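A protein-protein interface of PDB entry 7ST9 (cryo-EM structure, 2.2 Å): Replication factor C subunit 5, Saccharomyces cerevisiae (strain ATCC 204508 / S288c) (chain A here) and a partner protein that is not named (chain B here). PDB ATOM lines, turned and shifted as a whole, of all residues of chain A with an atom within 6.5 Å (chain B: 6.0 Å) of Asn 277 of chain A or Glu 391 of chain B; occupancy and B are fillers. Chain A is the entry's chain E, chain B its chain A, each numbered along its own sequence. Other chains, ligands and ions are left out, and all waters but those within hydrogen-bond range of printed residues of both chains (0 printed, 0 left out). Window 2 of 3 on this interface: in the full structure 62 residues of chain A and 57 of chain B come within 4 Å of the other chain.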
ATOM      1  N   SER A 275       2.020  18.185  25.602  1.00  0.00           N
ATOM      2  CA  SER A 275       2.646  17.205  26.481  1.00  0.00           C
ATOM      3  C   SER A 275       4.020  16.863  25.917  1.00  0.00           C
ATOM      4  O   SER A 275       4.405  17.326  24.840  1.00  0.00           O
ATOM      5  CB  SER A 275       1.774  15.955  26.627  1.00  0.00           C
ATOM      6  OG  SER A 275       1.730  15.220  25.418  1.00  0.00           O
ATOM      7  N   VAL A 276       4.762  16.043  26.665  1.00  0.00           N
ATOM      8  CA  VAL A 276       6.104  15.657  26.236  1.00  0.00           C
ATOM      9  C   VAL A 276       6.043  14.865  24.936  1.00  0.00           C
ATOM     10  O   VAL A 276       6.831  15.100  24.012  1.00  0.00           O
ATOM     11  CB  VAL A 276       6.811  14.866  27.352  1.00  0.00           C
ATOM     12  CG1 VAL A 276       8.215  14.470  26.919  1.00  0.00           C
ATOM     13  CG2 VAL A 276       6.856  15.682  28.636  1.00  0.00           C
ATOM     14  N   ASN A 277       5.110  13.914  24.843  1.00  0.00           N
ATOM     15  CA  ASN A 277       4.986  13.116  23.626  1.00  0.00           C
ATOM     16  C   ASN A 277       4.620  13.989  22.432  1.00  0.00           C
ATOM     17  O   ASN A 277       5.140  13.796  21.323  1.00  0.00           O
ATOM     18  CB  ASN A 277       3.941  12.019  23.829  1.00  0.00           C
ATOM     19  CG  ASN A 277       4.430  10.911  24.742  1.00  0.00           C
ATOM     20  OD1 ASN A 277       5.628  10.645  24.827  1.00  0.00           O
ATOM     21  ND2 ASN A 277       3.501  10.262  25.433  1.00  0.00           N
ATOM     22  N   SER A 278       3.716  14.947  22.636  1.00  0.00           N
ATOM     23  CA  SER A 278       3.408  15.901  21.579  1.00  0.00           C
ATOM     24  C   SER A 278       4.657  16.669  21.167  1.00  0.00           C
ATOM     25  O   SER A 278       4.864  16.943  19.981  1.00  0.00           O
ATOM     26  CB  SER A 278       2.314  16.862  22.041  1.00  0.00           C
ATOM     27  OG  SER A 278       1.040  16.244  21.991  1.00  0.00           O
ATOM     28  N   LEU A 279       5.505  17.019  22.137  1.00  0.00           N
ATOM     29  CA  LEU A 279       6.742  17.721  21.816  1.00  0.00           C
ATOM     30  C   LEU A 279       7.672  16.846  20.982  1.00  0.00           C
ATOM     31  O   LEU A 279       8.336  17.337  20.064  1.00  0.00           O
ATOM     32  CB  LEU A 279       7.433  18.176  23.101  1.00  0.00           C
ATOM     33  CG  LEU A 279       8.666  19.061  22.907  1.00  0.00           C
ATOM     34  CD1 LEU A 279       8.297  20.527  23.047  1.00  0.00           C
ATOM     35  CD2 LEU A 279       9.753  18.686  23.897  1.00  0.00           C
ATOM     36  N   ILE A 280       7.742  15.549  21.288  1.00  0.00           N
ATOM     37  CA  ILE A 280       8.581  14.652  20.498  1.00  0.00           C
ATOM     38  C   ILE A 280       8.051  14.544  19.071  1.00  0.00           C
ATOM     39  O   ILE A 280       8.822  14.533  18.102  1.00  0.00           O
ATOM     40  CB  ILE A 280       8.679  13.269  21.169  1.00  0.00           C
ATOM     41  CG1 ILE A 280       9.097  13.392  22.640  1.00  0.00           C
ATOM     42  CG2 ILE A 280       9.666  12.381  20.420  1.00  0.00           C
ATOM     43  CD1 ILE A 280      10.096  14.498  22.931  1.00  0.00           C
ATOM     44  N   GLU A 281       6.729  14.453  18.916  1.00  0.00           N
ATOM     45  CA  GLU A 281       6.153  14.418  17.573  1.00  0.00           C
ATOM     46  C   GLU A 281       6.447  15.712  16.818  1.00  0.00           C
ATOM     47  O   GLU A 281       6.766  15.690  15.619  1.00  0.00           O
ATOM     48  CB  GLU A 281       4.648  14.168  17.658  1.00  0.00           C
ATOM     49  CG  GLU A 281       4.286  12.736  18.022  1.00  0.00           C
ATOM     50  CD  GLU A 281       2.936  12.628  18.702  1.00  0.00           C
ATOM     51  OE1 GLU A 281       1.925  13.027  18.087  1.00  0.00           O
ATOM     52  OE2 GLU A 281       2.885  12.142  19.851  1.00  0.00           O
ATOM     53  N   CYS A 282       6.350  16.850  17.505  1.00  0.00           N
ATOM     54  CA  CYS A 282       6.690  18.123  16.882  1.00  0.00           C
ATOM     55  C   CYS A 282       8.158  18.156  16.474  1.00  0.00           C
ATOM     56  O   CYS A 282       8.505  18.714  15.429  1.00  0.00           O
ATOM     57  CB  CYS A 282       6.370  19.273  17.835  1.00  0.00           C
ATOM     58  SG  CYS A 282       4.603  19.583  18.058  1.00  0.00           S
ATOM     59  N   MET A 350       4.130  25.446  24.454  1.00  0.00           N
ATOM     60  CA  MET A 350       3.286  24.454  25.110  1.00  0.00           C
ATOM     61  C   MET A 350       3.072  24.802  26.577  1.00  0.00           C
ATOM     62  O   MET A 350       1.963  24.660  27.104  1.00  0.00           O
ATOM     63  CB  MET A 350       3.909  23.064  24.978  1.00  0.00           C
ATOM     64  CG  MET A 350       3.399  22.268  23.789  1.00  0.00           C
ATOM     65  SD  MET A 350       4.302  20.727  23.543  1.00  0.00           S
ATOM     66  CE  MET A 350       3.777  20.286  21.889  1.00  0.00           C
ATOM     67  N   ASN B 385      13.294  12.710  27.295  1.00  0.00           N
ATOM     68  CA  ASN B 385      11.890  12.320  27.368  1.00  0.00           C
ATOM     69  C   ASN B 385      11.710  10.872  27.803  1.00  0.00           C
ATOM     70  O   ASN B 385      10.604  10.492  28.201  1.00  0.00           O
ATOM     71  CB  ASN B 385      11.215  12.532  26.012  1.00  0.00           C
ATOM     72  CG  ASN B 385      11.716  11.567  24.956  1.00  0.00           C
ATOM     73  OD1 ASN B 385      12.877  11.619  24.554  1.00  0.00           O
ATOM     74  ND2 ASN B 385      10.840  10.680  24.502  1.00  0.00           N
ATOM     75  N   PHE B 387      12.597   9.579  30.436  1.00  0.00           N
ATOM     76  CA  PHE B 387      12.285   9.538  31.858  1.00  0.00           C
ATOM     77  C   PHE B 387      10.791   9.331  32.065  1.00  0.00           C
ATOM     78  O   PHE B 387       9.967  10.069  31.516  1.00  0.00           O
ATOM     79  CB  PHE B 387      12.739  10.835  32.528  1.00  0.00           C
ATOM     80  CG  PHE B 387      12.702  10.788  34.027  1.00  0.00           C
ATOM     81  CD1 PHE B 387      11.555  11.145  34.716  1.00  0.00           C
ATOM     82  CD2 PHE B 387      13.815  10.391  34.749  1.00  0.00           C
ATOM     83  CE1 PHE B 387      11.518  11.105  36.097  1.00  0.00           C
ATOM     84  CE2 PHE B 387      13.783  10.349  36.130  1.00  0.00           C
ATOM     85  CZ  PHE B 387      12.635  10.707  36.803  1.00  0.00           C
ATOM     86  N   ASN B 388      10.443   8.323  32.864  1.00  0.00           N
ATOM     87  CA  ASN B 388       9.050   7.980  33.144  1.00  0.00           C
ATOM     88  C   ASN B 388       8.257   7.741  31.861  1.00  0.00           C
ATOM     89  O   ASN B 388       7.029   7.864  31.850  1.00  0.00           O
ATOM     90  CB  ASN B 388       8.375   9.064  33.989  1.00  0.00           C
ATOM     91  CG  ASN B 388       7.145   8.557  34.717  1.00  0.00           C
ATOM     92  OD1 ASN B 388       6.979   7.354  34.917  1.00  0.00           O
ATOM     93  ND2 ASN B 388       6.272   9.476  35.115  1.00  0.00           N
ATOM     94  N   LYS B 389       8.944   7.395  30.772  1.00  0.00           N
ATOM     95  CA  LYS B 389       8.306   7.237  29.466  1.00  0.00           C
ATOM     96  C   LYS B 389       7.554   8.508  29.074  1.00  0.00           C
ATOM     97  O   LYS B 389       6.465   8.457  28.502  1.00  0.00           O
ATOM     98  CB  LYS B 389       7.371   6.025  29.449  1.00  0.00           C
ATOM     99  CG  LYS B 389       8.023   4.727  29.907  1.00  0.00           C
ATOM    100  CD  LYS B 389       8.389   3.836  28.727  1.00  0.00           C
ATOM    101  CE  LYS B 389       7.178   3.099  28.172  1.00  0.00           C
ATOM    102  NZ  LYS B 389       6.477   2.282  29.202  1.00  0.00           N
ATOM    103  N   GLY B 390       8.145   9.656  29.384  1.00  0.00           N
ATOM    104  CA  GLY B 390       7.543  10.934  29.046  1.00  0.00           C
ATOM    105  C   GLY B 390       6.230  11.213  29.744  1.00  0.00           C
ATOM    106  O   GLY B 390       5.268  11.643  29.096  1.00  0.00           O
ATOM    107  N   GLU B 391       6.163  10.978  31.054  1.00  0.00           N
ATOM    108  CA  GLU B 391       4.962  11.215  31.846  1.00  0.00           C
ATOM    109  C   GLU B 391       5.239  12.204  32.974  1.00  0.00           C
ATOM    110  O   GLU B 391       4.776  12.037  34.104  1.00  0.00           O
ATOM    111  CB  GLU B 391       4.412   9.900  32.396  1.00  0.00           C
ATOM    112  CG  GLU B 391       3.272   9.322  31.576  1.00  0.00           C
ATOM    113  CD  GLU B 391       3.706   8.900  30.186  1.00  0.00           C
ATOM    114  OE1 GLU B 391       4.445   7.900  30.071  1.00  0.00           O
ATOM    115  OE2 GLU B 391       3.309   9.569  29.210  1.00  0.00           O
ATOM    116  N   PHE B 392       6.000  13.253  32.676  1.00  0.00           N
ATOM    117  CA  PHE B 392       6.262  14.332  33.617  1.00  0.00           C
ATOM    118  C   PHE B 392       5.765  15.648  33.031  1.00  0.00           C
ATOM    119  O   PHE B 392       5.371  15.730  31.866  1.00  0.00           O
ATOM    120  CB  PHE B 392       7.756  14.421  33.965  1.00  0.00           C
ATOM    121  CG  PHE B 392       8.665  14.408  32.769  1.00  0.00           C
ATOM    122  CD1 PHE B 392       9.056  13.211  32.192  1.00  0.00           C
ATOM    123  CD2 PHE B 392       9.139  15.591  32.230  1.00  0.00           C
ATOM    124  CE1 PHE B 392       9.897  13.197  31.096  1.00  0.00           C
ATOM    125  CE2 PHE B 392       9.980  15.582  31.135  1.00  0.00           C
ATOM    126  CZ  PHE B 392      10.358  14.383  30.568  1.00  0.00           C
ATOM    127  N   SER B 393       5.785  16.687  33.862  1.00  0.00           N
ATOM    128  CA  SER B 393       5.221  17.969  33.465  1.00  0.00           C
ATOM    129  C   SER B 393       6.000  18.568  32.299  1.00  0.00           C
ATOM    130  O   SER B 393       7.214  18.389  32.171  1.00  0.00           O
ATOM    131  CB  SER B 393       5.225  18.941  34.647  1.00  0.00           C
ATOM    132  OG  SER B 393       6.545  19.216  35.079  1.00  0.00           O
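Hydrophobic or aromatic side chains of chain A within 4 Å of the printed part of chain B: Val 276 and Ile 280. Among the printed residues, no Asp or Glu carboxylate lies within 4 Å of a Lys or Arg side-chain nitrogen of the other chain.
Of the printed residues of chain B, Val 276 of chain A touches Asn 385 (3.7 Å), Gly 390 (3.98 Å) and Phe 392 (3.6 Å). Of chain B, only Glu 391 (3.8 Å) comes within 4 Å of Asn 277 of chain A. Leu 279 of chain A touches none of the printed residues of chain B. Of chain A, only Asn 277 (3.8 Å) comes within 4 Å of Glu 391 of chain B. Of the printed residues of chain A, Phe 392 of chain B touches Val 276 (3.6 Å). The nearest residue of chain A that does not touch Glu 391 of chain B is Val 276 of chain A (5.3 Å). The nearest printed residue of chain A that does not touch Asn 385 of chain B is Asn 277 of chain A (5.2 Å).
Among the printed residues, merely in contact across the chains: Val 276 of chain A with Asn 385 of chain B, Val 276 of chain A with Gly 390 of chain B, Val 276 of chain A with Phe 392 of chain B, Asn 277 of chain A with Glu 391 of chain B and Ile 280 of chain A with Asn 385 of chain B.
The backbone carbonyl oxygen of Asn 385 of chain B sits at hydrogen-bond distance from the backbone NH of Gly 390 of chain B (2.9 Å). O of Glu 391 of chain B sits at hydrogen-bond distance from ND2 of Asn 388 of chain B (3.1 Å). O of Lys 389 of chain B lies close to OE1 of Glu 391 of chain B (2.6 Å).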
